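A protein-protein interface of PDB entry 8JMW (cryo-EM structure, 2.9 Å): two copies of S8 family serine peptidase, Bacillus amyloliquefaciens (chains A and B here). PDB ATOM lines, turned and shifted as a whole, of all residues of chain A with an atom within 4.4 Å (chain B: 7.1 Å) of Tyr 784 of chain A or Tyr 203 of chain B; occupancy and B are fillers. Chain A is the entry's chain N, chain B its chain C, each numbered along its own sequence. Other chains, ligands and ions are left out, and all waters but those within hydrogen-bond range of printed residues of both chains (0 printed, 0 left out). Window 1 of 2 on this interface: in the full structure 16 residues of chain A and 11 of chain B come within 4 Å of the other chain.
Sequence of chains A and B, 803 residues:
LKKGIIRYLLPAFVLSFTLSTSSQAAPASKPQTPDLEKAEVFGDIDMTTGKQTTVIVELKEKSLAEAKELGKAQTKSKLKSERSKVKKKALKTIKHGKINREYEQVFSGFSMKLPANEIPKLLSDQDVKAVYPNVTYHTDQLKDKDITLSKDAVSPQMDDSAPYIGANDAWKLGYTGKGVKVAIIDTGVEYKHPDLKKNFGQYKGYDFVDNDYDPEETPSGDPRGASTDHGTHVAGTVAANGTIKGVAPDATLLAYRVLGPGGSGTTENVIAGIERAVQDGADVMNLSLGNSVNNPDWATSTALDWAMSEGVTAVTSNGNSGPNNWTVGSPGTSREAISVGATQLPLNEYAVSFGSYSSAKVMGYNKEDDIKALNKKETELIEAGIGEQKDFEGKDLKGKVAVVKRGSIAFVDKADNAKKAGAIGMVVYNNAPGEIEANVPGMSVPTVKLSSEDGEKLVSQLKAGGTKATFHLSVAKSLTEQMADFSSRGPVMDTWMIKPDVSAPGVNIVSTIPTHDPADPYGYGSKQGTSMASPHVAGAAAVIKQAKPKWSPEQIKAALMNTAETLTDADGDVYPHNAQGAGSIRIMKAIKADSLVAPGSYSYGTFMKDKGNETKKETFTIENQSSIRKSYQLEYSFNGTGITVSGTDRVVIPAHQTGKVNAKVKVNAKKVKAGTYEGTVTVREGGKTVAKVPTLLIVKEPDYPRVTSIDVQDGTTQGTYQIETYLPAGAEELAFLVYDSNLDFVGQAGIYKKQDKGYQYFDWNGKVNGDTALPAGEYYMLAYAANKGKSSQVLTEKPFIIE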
ATOM      1  N   GLU A 733     -30.491 -17.295  -1.735  1.00  0.00           N
ATOM      2  CA  GLU A 733     -29.600 -16.149  -1.809  1.00  0.00           C
ATOM      3  C   GLU A 733     -28.247 -16.536  -1.242  1.00  0.00           C
ATOM      4  O   GLU A 733     -28.171 -17.239  -0.235  1.00  0.00           O
ATOM      5  CB  GLU A 733     -30.176 -14.953  -1.052  1.00  0.00           C
ATOM      6  CG  GLU A 733     -29.343 -13.696  -1.139  1.00  0.00           C
ATOM      7  CD  GLU A 733     -29.978 -12.528  -0.415  1.00  0.00           C
ATOM      8  OE1 GLU A 733     -31.055 -12.714   0.189  1.00  0.00           O
ATOM      9  OE2 GLU A 733     -29.399 -11.421  -0.447  1.00  0.00           O
ATOM     10  N   LEU A 734     -27.179 -16.091  -1.892  1.00  0.00           N
ATOM     11  CA  LEU A 734     -25.827 -16.409  -1.466  1.00  0.00           C
ATOM     12  C   LEU A 734     -24.990 -15.144  -1.504  1.00  0.00           C
ATOM     13  O   LEU A 734     -25.009 -14.417  -2.498  1.00  0.00           O
ATOM     14  CB  LEU A 734     -25.218 -17.486  -2.359  1.00  0.00           C
ATOM     15  CG  LEU A 734     -23.765 -17.860  -2.106  1.00  0.00           C
ATOM     16  CD1 LEU A 734     -23.618 -18.465  -0.737  1.00  0.00           C
ATOM     17  CD2 LEU A 734     -23.321 -18.838  -3.151  1.00  0.00           C
ATOM     18  N   ALA A 735     -24.269 -14.874  -0.428  1.00  0.00           N
ATOM     19  CA  ALA A 735     -23.490 -13.654  -0.321  1.00  0.00           C
ATOM     20  C   ALA A 735     -22.097 -13.972   0.182  1.00  0.00           C
ATOM     21  O   ALA A 735     -21.932 -14.728   1.140  1.00  0.00           O
ATOM     22  CB  ALA A 735     -24.157 -12.656   0.615  1.00  0.00           C
ATOM     23  N   TYR A 739     -13.543  -9.922   5.179  1.00  0.00           N
ATOM     24  CA  TYR A 739     -13.106  -9.418   6.469  1.00  0.00           C
ATOM     25  C   TYR A 739     -11.592  -9.287   6.471  1.00  0.00           C
ATOM     26  O   TYR A 739     -10.889 -10.065   5.826  1.00  0.00           O
ATOM     27  CB  TYR A 739     -13.546 -10.347   7.595  1.00  0.00           C
ATOM     28  CG  TYR A 739     -15.036 -10.414   7.746  1.00  0.00           C
ATOM     29  CD1 TYR A 739     -15.707  -9.499   8.531  1.00  0.00           C
ATOM     30  CD2 TYR A 739     -15.772 -11.396   7.113  1.00  0.00           C
ATOM     31  CE1 TYR A 739     -17.067  -9.559   8.682  1.00  0.00           C
ATOM     32  CE2 TYR A 739     -17.133 -11.463   7.257  1.00  0.00           C
ATOM     33  CZ  TYR A 739     -17.774 -10.542   8.043  1.00  0.00           C
ATOM     34  OH  TYR A 739     -19.136 -10.603   8.192  1.00  0.00           O
ATOM     35  N   LEU A 782     -16.542 -14.780   4.288  1.00  0.00           N
ATOM     36  CA  LEU A 782     -17.702 -15.394   4.908  1.00  0.00           C
ATOM     37  C   LEU A 782     -18.748 -15.642   3.837  1.00  0.00           C
ATOM     38  O   LEU A 782     -19.094 -14.730   3.080  1.00  0.00           O
ATOM     39  CB  LEU A 782     -18.282 -14.498   5.999  1.00  0.00           C
ATOM     40  CG  LEU A 782     -19.546 -15.020   6.674  1.00  0.00           C
ATOM     41  CD1 LEU A 782     -19.214 -16.198   7.549  1.00  0.00           C
ATOM     42  CD2 LEU A 782     -20.218 -13.936   7.473  1.00  0.00           C
ATOM     43  N   ALA A 783     -19.235 -16.871   3.768  1.00  0.00           N
ATOM     44  CA  ALA A 783     -20.330 -17.223   2.883  1.00  0.00           C
ATOM     45  C   ALA A 783     -21.607 -17.288   3.700  1.00  0.00           C
ATOM     46  O   ALA A 783     -21.666 -17.998   4.707  1.00  0.00           O
ATOM     47  CB  ALA A 783     -20.080 -18.559   2.192  1.00  0.00           C
ATOM     48  N   TYR A 784     -22.610 -16.535   3.274  1.00  0.00           N
ATOM     49  CA  TYR A 784     -23.914 -16.497   3.917  1.00  0.00           C
ATOM     50  C   TYR A 784     -24.930 -17.005   2.909  1.00  0.00           C
ATOM     51  O   TYR A 784     -25.164 -16.361   1.885  1.00  0.00           O
ATOM     52  CB  TYR A 784     -24.251 -15.081   4.375  1.00  0.00           C
ATOM     53  CG  TYR A 784     -25.687 -14.906   4.778  1.00  0.00           C
ATOM     54  CD1 TYR A 784     -26.095 -15.170   6.069  1.00  0.00           C
ATOM     55  CD2 TYR A 784     -26.637 -14.482   3.867  1.00  0.00           C
ATOM     56  CE1 TYR A 784     -27.402 -15.018   6.439  1.00  0.00           C
ATOM     57  CE2 TYR A 784     -27.946 -14.332   4.229  1.00  0.00           C
ATOM     58  CZ  TYR A 784     -28.324 -14.599   5.517  1.00  0.00           C
ATOM     59  OH  TYR A 784     -29.635 -14.445   5.888  1.00  0.00           O
ATOM     60  N   ALA A 785     -25.527 -18.154   3.187  1.00  0.00           N
ATOM     61  CA  ALA A 785     -26.506 -18.752   2.298  1.00  0.00           C
ATOM     62  C   ALA A 785     -27.855 -18.822   2.990  1.00  0.00           C
ATOM     63  O   ALA A 785     -27.957 -19.296   4.122  1.00  0.00           O
ATOM     64  CB  ALA A 785     -26.074 -20.149   1.864  1.00  0.00           C
ATOM     65  N   ALA A 786     -28.888 -18.357   2.304  1.00  0.00           N
ATOM     66  CA  ALA A 786     -30.250 -18.396   2.807  1.00  0.00           C
ATOM     67  C   ALA A 786     -31.087 -19.232   1.858  1.00  0.00           C
ATOM     68  O   ALA A 786     -31.078 -18.994   0.645  1.00  0.00           O
ATOM     69  CB  ALA A 786     -30.839 -16.993   2.934  1.00  0.00           C
ATOM     70  N   SER A 791     -31.063 -19.535   7.268  1.00  0.00           N
ATOM     71  CA  SER A 791     -29.804 -19.042   6.745  1.00  0.00           C
ATOM     72  C   SER A 791     -28.663 -19.581   7.582  1.00  0.00           C
ATOM     73  O   SER A 791     -28.795 -19.784   8.789  1.00  0.00           O
ATOM     74  CB  SER A 791     -29.754 -17.528   6.741  1.00  0.00           C
ATOM     75  OG  SER A 791     -29.417 -17.040   8.023  1.00  0.00           O
ATOM     76  N   SER A 792     -27.536 -19.806   6.922  1.00  0.00           N
ATOM     77  CA  SER A 792     -26.339 -20.308   7.566  1.00  0.00           C
ATOM     78  C   SER A 792     -25.149 -19.551   7.011  1.00  0.00           C
ATOM     79  O   SER A 792     -25.233 -18.908   5.967  1.00  0.00           O
ATOM     80  CB  SER A 792     -26.163 -21.810   7.344  1.00  0.00           C
ATOM     81  OG  SER A 792     -26.956 -22.549   8.252  1.00  0.00           O
ATOM     82  N   GLN A 793     -24.039 -19.616   7.733  1.00  0.00           N
ATOM     83  CA  GLN A 793     -22.834 -18.928   7.316  1.00  0.00           C
ATOM     84  C   GLN A 793     -21.629 -19.775   7.668  1.00  0.00           C
ATOM     85  O   GLN A 793     -21.668 -20.587   8.592  1.00  0.00           O
ATOM     86  CB  GLN A 793     -22.716 -17.559   7.970  1.00  0.00           C
ATOM     87  CG  GLN A 793     -22.784 -17.614   9.464  1.00  0.00           C
ATOM     88  CD  GLN A 793     -23.424 -16.391  10.048  1.00  0.00           C
ATOM     89  OE1 GLN A 793     -24.537 -16.027   9.677  1.00  0.00           O
ATOM     90  NE2 GLN A 793     -22.732 -15.746  10.974  1.00  0.00           N
ATOM     91  N   LYS B 181     -29.395 -14.635  20.759  1.00  0.00           N
ATOM     92  CA  LYS B 181     -29.188 -13.770  19.605  1.00  0.00           C
ATOM     93  C   LYS B 181     -30.344 -12.783  19.532  1.00  0.00           C
ATOM     94  O   LYS B 181     -31.513 -13.186  19.490  1.00  0.00           O
ATOM     95  CB  LYS B 181     -29.072 -14.598  18.332  1.00  0.00           C
ATOM     96  CG  LYS B 181     -28.457 -13.859  17.173  1.00  0.00           C
ATOM     97  CD  LYS B 181     -27.506 -14.750  16.395  1.00  0.00           C
ATOM     98  CE  LYS B 181     -27.944 -16.201  16.422  1.00  0.00           C
ATOM     99  NZ  LYS B 181     -27.555 -16.913  15.178  1.00  0.00           N
ATOM    100  N   PHE B 200     -21.162  -8.091  18.333  1.00  0.00           N
ATOM    101  CA  PHE B 200     -21.549  -8.417  16.971  1.00  0.00           C
ATOM    102  C   PHE B 200     -20.714  -9.575  16.455  1.00  0.00           C
ATOM    103  O   PHE B 200     -19.489  -9.584  16.602  1.00  0.00           O
ATOM    104  CB  PHE B 200     -21.385  -7.201  16.068  1.00  0.00           C
ATOM    105  CG  PHE B 200     -22.579  -6.313  16.052  1.00  0.00           C
ATOM    106  CD1 PHE B 200     -23.615  -6.549  15.176  1.00  0.00           C
ATOM    107  CD2 PHE B 200     -22.677  -5.252  16.923  1.00  0.00           C
ATOM    108  CE1 PHE B 200     -24.717  -5.740  15.163  1.00  0.00           C
ATOM    109  CE2 PHE B 200     -23.778  -4.441  16.912  1.00  0.00           C
ATOM    110  CZ  PHE B 200     -24.799  -4.686  16.032  1.00  0.00           C
ATOM    111  N   GLY B 201     -21.376 -10.550  15.848  1.00  0.00           N
ATOM    112  CA  GLY B 201     -20.670 -11.680  15.284  1.00  0.00           C
ATOM    113  C   GLY B 201     -20.023 -11.330  13.966  1.00  0.00           C
ATOM    114  O   GLY B 201     -19.800 -10.154  13.669  1.00  0.00           O
ATOM    115  N   GLN B 202     -19.703 -12.341  13.163  1.00  0.00           N
ATOM    116  CA  GLN B 202     -19.099 -12.079  11.865  1.00  0.00           C
ATOM    117  C   GLN B 202     -20.117 -11.411  10.956  1.00  0.00           C
ATOM    118  O   GLN B 202     -19.858 -10.348  10.385  1.00  0.00           O
ATOM    119  CB  GLN B 202     -18.556 -13.379  11.274  1.00  0.00           C
ATOM    120  CG  GLN B 202     -17.332 -13.899  11.988  1.00  0.00           C
ATOM    121  CD  GLN B 202     -16.203 -12.896  12.027  1.00  0.00           C
ATOM    122  OE1 GLN B 202     -16.143 -11.970  11.222  1.00  0.00           O
ATOM    123  NE2 GLN B 202     -15.313 -13.060  12.992  1.00  0.00           N
ATOM    124  N   TYR B 203     -21.286 -12.020  10.818  1.00  0.00           N
ATOM    125  CA  TYR B 203     -22.359 -11.469  10.005  1.00  0.00           C
ATOM    126  C   TYR B 203     -23.167 -10.479  10.830  1.00  0.00           C
ATOM    127  O   TYR B 203     -23.809 -10.861  11.812  1.00  0.00           O
ATOM    128  CB  TYR B 203     -23.230 -12.607   9.481  1.00  0.00           C
ATOM    129  CG  TYR B 203     -24.592 -12.201   8.995  1.00  0.00           C
ATOM    130  CD1 TYR B 203     -24.765 -11.658   7.738  1.00  0.00           C
ATOM    131  CD2 TYR B 203     -25.710 -12.396   9.781  1.00  0.00           C
ATOM    132  CE1 TYR B 203     -26.009 -11.302   7.288  1.00  0.00           C
ATOM    133  CE2 TYR B 203     -26.955 -12.043   9.340  1.00  0.00           C
ATOM    134  CZ  TYR B 203     -27.100 -11.498   8.094  1.00  0.00           C
ATOM    135  OH  TYR B 203     -28.348 -11.144   7.650  1.00  0.00           O
ATOM    136  N   LYS B 204     -23.123  -9.208  10.442  1.00  0.00           N
ATOM    137  CA  LYS B 204     -23.704  -8.152  11.257  1.00  0.00           C
ATOM    138  C   LYS B 204     -25.195  -7.974  11.036  1.00  0.00           C
ATOM    139  O   LYS B 204     -25.899  -7.541  11.953  1.00  0.00           O
ATOM    140  CB  LYS B 204     -22.988  -6.831  10.989  1.00  0.00           C
ATOM    141  CG  LYS B 204     -21.522  -7.004  10.694  1.00  0.00           C
ATOM    142  CD  LYS B 204     -20.724  -6.945  11.973  1.00  0.00           C
ATOM    143  CE  LYS B 204     -19.244  -6.876  11.697  1.00  0.00           C
ATOM    144  NZ  LYS B 204     -18.476  -7.606  12.734  1.00  0.00           N
ATOM    145  N   GLY B 205     -25.694  -8.293   9.863  1.00  0.00           N
ATOM    146  CA  GLY B 205     -27.100  -8.128   9.579  1.00  0.00           C
ATOM    147  C   GLY B 205     -27.292  -7.739   8.132  1.00  0.00           C
ATOM    148  O   GLY B 205     -26.470  -8.037   7.275  1.00  0.00           O
ATOM    149  N   TYR B 206     -28.398  -7.057   7.882  1.00  0.00           N
ATOM    150  CA  TYR B 206     -28.766  -6.670   6.533  1.00  0.00           C
ATOM    151  C   TYR B 206     -29.308  -5.250   6.517  1.00  0.00           C
ATOM    152  O   TYR B 206     -29.777  -4.731   7.533  1.00  0.00           O
ATOM    153  CB  TYR B 206     -29.794  -7.635   5.952  1.00  0.00           C
ATOM    154  CG  TYR B 206     -29.913  -7.574   4.453  1.00  0.00           C
ATOM    155  CD1 TYR B 206     -28.819  -7.806   3.645  1.00  0.00           C
ATOM    156  CD2 TYR B 206     -31.121  -7.300   3.847  1.00  0.00           C
ATOM    157  CE1 TYR B 206     -28.926  -7.753   2.279  1.00  0.00           C
ATOM    158  CE2 TYR B 206     -31.236  -7.246   2.484  1.00  0.00           C
ATOM    159  CZ  TYR B 206     -30.138  -7.473   1.704  1.00  0.00           C
ATOM    160  OH  TYR B 206     -30.251  -7.421   0.339  1.00  0.00           O
ATOM    161  N   ASP B 207     -29.234  -4.625   5.353  1.00  0.00           N
ATOM    162  CA  ASP B 207     -29.616  -3.233   5.167  1.00  0.00           C
ATOM    163  C   ASP B 207     -30.657  -3.201   4.057  1.00  0.00           C
ATOM    164  O   ASP B 207     -30.311  -3.187   2.875  1.00  0.00           O
ATOM    165  CB  ASP B 207     -28.389  -2.397   4.837  1.00  0.00           C
ATOM    166  CG  ASP B 207     -28.699  -0.939   4.620  1.00  0.00           C
ATOM    167  OD1 ASP B 207     -29.878  -0.549   4.680  1.00  0.00           O
ATOM    168  OD2 ASP B 207     -27.744  -0.172   4.387  1.00  0.00           O
ATOM    169  N   TYR B 213     -24.954  -5.615   2.756  1.00  0.00           N
ATOM    170  CA  TYR B 213     -24.705  -6.277   4.029  1.00  0.00           C
ATOM    171  C   TYR B 213     -23.986  -5.381   5.019  1.00  0.00           C
ATOM    172  O   TYR B 213     -23.250  -5.874   5.881  1.00  0.00           O
ATOM    173  CB  TYR B 213     -23.928  -7.567   3.796  1.00  0.00           C
ATOM    174  CG  TYR B 213     -24.813  -8.676   3.308  1.00  0.00           C
ATOM    175  CD1 TYR B 213     -25.246  -8.709   1.998  1.00  0.00           C
ATOM    176  CD2 TYR B 213     -25.237  -9.674   4.161  1.00  0.00           C
ATOM    177  CE1 TYR B 213     -26.064  -9.711   1.548  1.00  0.00           C
ATOM    178  CE2 TYR B 213     -26.054 -10.678   3.721  1.00  0.00           C
ATOM    179  CZ  TYR B 213     -26.465 -10.693   2.414  1.00  0.00           C
ATOM    180  OH  TYR B 213     -27.282 -11.698   1.968  1.00  0.00           O
ATOM    181  N   PRO B 215     -25.194  -2.724   7.595  1.00  0.00           N
ATOM    182  CA  PRO B 215     -26.294  -2.035   8.279  1.00  0.00           C
ATOM    183  C   PRO B 215     -25.836  -0.842   9.114  1.00  0.00           C
ATOM    184  O   PRO B 215     -26.252  -0.665  10.256  1.00  0.00           O
ATOM    185  CB  PRO B 215     -26.888  -3.136   9.162  1.00  0.00           C
ATOM    186  CG  PRO B 215     -26.167  -4.398   8.799  1.00  0.00           C
ATOM    187  CD  PRO B 215     -24.855  -3.981   8.267  1.00  0.00           C
ATOM    188  N   THR B 252     -25.416 -11.946  21.404  1.00  0.00           N
ATOM    189  CA  THR B 252     -25.057 -11.612  20.039  1.00  0.00           C
ATOM    190  C   THR B 252     -26.106 -10.681  19.453  1.00  0.00           C
ATOM    191  O   THR B 252     -27.288 -10.756  19.791  1.00  0.00           O
ATOM    192  CB  THR B 252     -24.941 -12.876  19.193  1.00  0.00           C
ATOM    193  OG1 THR B 252     -24.299 -13.901  19.957  1.00  0.00           O
ATOM    194  CG2 THR B 252     -24.125 -12.608  17.945  1.00  0.00           C
ATOM    195  N   LEU B 253     -25.666  -9.796  18.567  1.00  0.00           N
ATOM    196  CA  LEU B 253     -26.542  -8.786  18.001  1.00  0.00           C
ATOM    197  C   LEU B 253     -26.584  -8.919  16.490  1.00  0.00           C
ATOM    198  O   LEU B 253     -25.588  -9.280  15.862  1.00  0.00           O
ATOM    199  CB  LEU B 253     -26.079  -7.384  18.376  1.00  0.00           C
ATOM    200  CG  LEU B 253     -26.450  -6.904  19.772  1.00  0.00           C
ATOM    201  CD1 LEU B 253     -25.484  -5.837  20.221  1.00  0.00           C
ATOM    202  CD2 LEU B 253     -27.863  -6.380  19.785  1.00  0.00           C
ATOM    203  N   LEU B 254     -27.747  -8.633  15.917  1.00  0.00           N
ATOM    204  CA  LEU B 254     -27.913  -8.527  14.475  1.00  0.00           C
ATOM    205  C   LEU B 254     -28.618  -7.218  14.176  1.00  0.00           C
ATOM    206  O   LEU B 254     -29.605  -6.881  14.832  1.00  0.00           O
ATOM    207  CB  LEU B 254     -28.714  -9.696  13.911  1.00  0.00           C
ATOM    208  CG  LEU B 254     -28.255 -11.101  14.279  1.00  0.00           C
ATOM    209  CD1 LEU B 254     -29.422 -12.054  14.210  1.00  0.00           C
ATOM    210  CD2 LEU B 254     -27.159 -11.541  13.345  1.00  0.00           C
ATOM    211  N   ALA B 255     -28.115  -6.485  13.194  1.00  0.00           N
ATOM    212  CA  ALA B 255     -28.690  -5.209  12.815  1.00  0.00           C
ATOM    213  C   ALA B 255     -29.428  -5.332  11.492  1.00  0.00           C
ATOM    214  O   ALA B 255     -28.933  -5.933  10.536  1.00  0.00           O
ATOM    215  CB  ALA B 255     -27.609  -4.137  12.706  1.00  0.00           C
ATOM    216  N   TYR B 256     -30.618  -4.748  11.441  1.00  0.00           N
ATOM    217  CA  TYR B 256     -31.441  -4.793  10.238  1.00  0.00           C
ATOM    218  C   TYR B 256     -31.923  -3.376   9.967  1.00  0.00           C
ATOM    219  O   TYR B 256     -32.848  -2.891  10.621  1.00  0.00           O
ATOM    220  CB  TYR B 256     -32.597  -5.762  10.401  1.00  0.00           C
ATOM    221  CG  TYR B 256     -32.123  -7.177  10.533  1.00  0.00           C
ATOM    222  CD1 TYR B 256     -31.505  -7.817   9.481  1.00  0.00           C
ATOM    223  CD2 TYR B 256     -32.264  -7.863  11.720  1.00  0.00           C
ATOM    224  CE1 TYR B 256     -31.054  -9.098   9.601  1.00  0.00           C
ATOM    225  CE2 TYR B 256     -31.816  -9.147  11.848  1.00  0.00           C
ATOM    226  CZ  TYR B 256     -31.214  -9.758  10.785  1.00  0.00           C
ATOM    227  OH  TYR B 256     -30.764 -11.045  10.909  1.00  0.00           O
ATOM    228  N   ARG B 276     -36.435 -11.796   7.839  1.00  0.00           N
ATOM    229  CA  ARG B 276     -35.015 -12.095   7.755  1.00  0.00           C
ATOM    230  C   ARG B 276     -34.407 -12.305   9.132  1.00  0.00           C
ATOM    231  O   ARG B 276     -33.500 -13.127   9.282  1.00  0.00           O
ATOM    232  CB  ARG B 276     -34.301 -10.973   7.005  1.00  0.00           C
ATOM    233  CG  ARG B 276     -32.832 -10.861   7.283  1.00  0.00           C
ATOM    234  CD  ARG B 276     -32.064 -11.902   6.516  1.00  0.00           C
ATOM    235  NE  ARG B 276     -32.039 -11.618   5.089  1.00  0.00           N
ATOM    236  CZ  ARG B 276     -30.942 -11.336   4.405  1.00  0.00           C
ATOM    237  NH1 ARG B 276     -29.757 -11.285   4.989  1.00  0.00           N
ATOM    238  NH2 ARG B 276     -31.034 -11.105   3.100  1.00  0.00           N
ATOM    239  N   ALA B 277     -34.897 -11.595  10.147  1.00  0.00           N
ATOM    240  CA  ALA B 277     -34.443 -11.855  11.505  1.00  0.00           C
ATOM    241  C   ALA B 277     -34.857 -13.237  11.971  1.00  0.00           C
ATOM    242  O   ALA B 277     -34.110 -13.894  12.700  1.00  0.00           O
ATOM    243  CB  ALA B 277     -34.988 -10.797  12.456  1.00  0.00           C
ATOM    244  N   GLN B 279     -35.186 -15.735   9.893  1.00  0.00           N
ATOM    245  CA  GLN B 279     -34.255 -16.576   9.146  1.00  0.00           C
ATOM    246  C   GLN B 279     -32.940 -16.738   9.888  1.00  0.00           C
ATOM    247  O   GLN B 279     -32.447 -17.855  10.071  1.00  0.00           O
ATOM    248  CB  GLN B 279     -33.982 -15.974   7.773  1.00  0.00           C
ATOM    249  CG  GLN B 279     -34.829 -16.495   6.660  1.00  0.00           C
ATOM    250  CD  GLN B 279     -34.227 -16.169   5.319  1.00  0.00           C
ATOM    251  OE1 GLN B 279     -33.155 -15.572   5.240  1.00  0.00           O
ATOM    252  NE2 GLN B 279     -34.906 -16.562   4.251  1.00  0.00           N
ATOM    253  N   ASP B 280     -32.358 -15.630  10.323  1.00  0.00           N
ATOM    254  CA  ASP B 280     -31.009 -15.626  10.859  1.00  0.00           C
ATOM    255  C   ASP B 280     -30.914 -16.231  12.245  1.00  0.00           C
ATOM    256  O   ASP B 280     -29.864 -16.107  12.879  1.00  0.00           O
ATOM    257  CB  ASP B 280     -30.483 -14.199  10.877  1.00  0.00           C
ATOM    258  CG  ASP B 280     -30.190 -13.682   9.493  1.00  0.00           C
ATOM    259  OD1 ASP B 280     -30.198 -14.495   8.548  1.00  0.00           O
ATOM    260  OD2 ASP B 280     -29.969 -12.467   9.342  1.00  0.00           O
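The side-chain hydroxyl (OH) of Tyr 739 of chain A lies close to the backbone carbonyl oxygen (O) of Gln 202 of chain B.
The side-chain carboxylate (OE1) of Glu 733 of chain A is in salt-bridge range of the guanidinium group (NH2) of Arg 276 of chain B (3.3 Å).
The side-chain carboxylate (OD1) of Asp 280 of chain B is in hydrogen-bond range of the side-chain hydroxyl (OH) of Tyr 784 of chain A, 2.7 Å away.
OH of Tyr 213 of chain B is in hydrogen-bond range of OE2 of Glu 733 of chain A, 3.2 Å away.
The side-chain hydroxyl (OG) of Ser 791 of chain A sits at hydrogen-bond distance from the side-chain carboxylate (OD1) of Asp 280 of chain B.
The guanidinium group (NH1) of Arg 276 of chain B is in hydrogen-bond range of the side-chain hydroxyl (OH) of Tyr 784 of chain A, at 3.3 Å.
The side-chain amino group (NZ) of Lys 181 of chain B is in hydrogen-bond range of the backbone carbonyl oxygen (O) of Asp 280 of chain B, at 3.4 Å.
O of Glu 733 of chain A is in hydrogen-bond range of N of Ala 786 of chain A (2.9 Å).
OH of Tyr 203 of chain B sits at hydrogen-bond distance from OD2 of Asp 280 of chain B, at 2.7 Å.
OH of Tyr 784 of chain A lies close to OG of Ser 791 of chain A (3.4 Å).
The backbone carbonyl oxygen (O) of Ala 735 of chain A is in hydrogen-bond range of the backbone NH (N) of Tyr 784 of chain A, at 2.9 Å.
The side-chain hydroxyl (OH) of Tyr 203 of chain B lies within hydrogen-bond range of the guanidinium group (NH1) of Arg 276 of chain B, 3.0 Å away.
CZ of Tyr 213 of chain B touches CB of Ala 735 of chain A, at 3.5 Å.
Tyr 739 of chain A touches Tyr 203 of chain B (OH to N, 3.7 Å).
Tyr 203 of chain B touches Leu 782 of chain A (CB to CD2, 3.9 Å).
CE1 of Tyr 784 of chain A touches CZ of Tyr 203 of chain B, at 3.9 Å.
CD2 of Tyr 784 of chain A touches OH of Tyr 213 of chain B (3.4 Å).
OE1 of Gln 279 of chain B touches OH of Tyr 784 of chain A, 3.8 Å away.
CB of Ala 786 of chain A touches OE1 of Gln 279 of chain B, 3.6 Å away.
Ser 791 of chain A touches Gln 279 of chain B.
CB of Tyr 203 of chain B touches NE2 of Gln 793 of chain A, at 3.5 Å.
Printed residues of chain B within 4 Å of Tyr 784 of chain A: Tyr 203 (3.9 Å), Tyr 213 (3.4 Å), Arg 276 (3.3 Å), Gln 279 (3.8 Å) and Asp 280 (2.7 Å).
Tyr 203 of chain B touches four residues of chain A.
Of the printed residues of chain A, Gln 202 of chain B touches Tyr 739 (2.3 Å).
Of the printed residues of chain B, Gln 793 of chain A touches Tyr 203.
Of the printed residues of chain B, Glu 733 of chain A touches Tyr 213 (3.2 Å) and Arg 276 (3.3 Å).
Of the printed residues of chain B, Ser 791 of chain A touches Gln 279 and Asp 280.
Printed residues of chain A within 4 Å of Asp 280 of chain B: Tyr 784 and Ser 791.
Hydrophobic or aromatic side chains of chain B within 4 Å of the printed part of chain A: Tyr 203 and Tyr 213.
Of the 12 printed residues of chain A, 8 touch a printed residue of chain B.
Among the printed residues, 15 pairs touch across the chains.
No position is printed for both chains.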
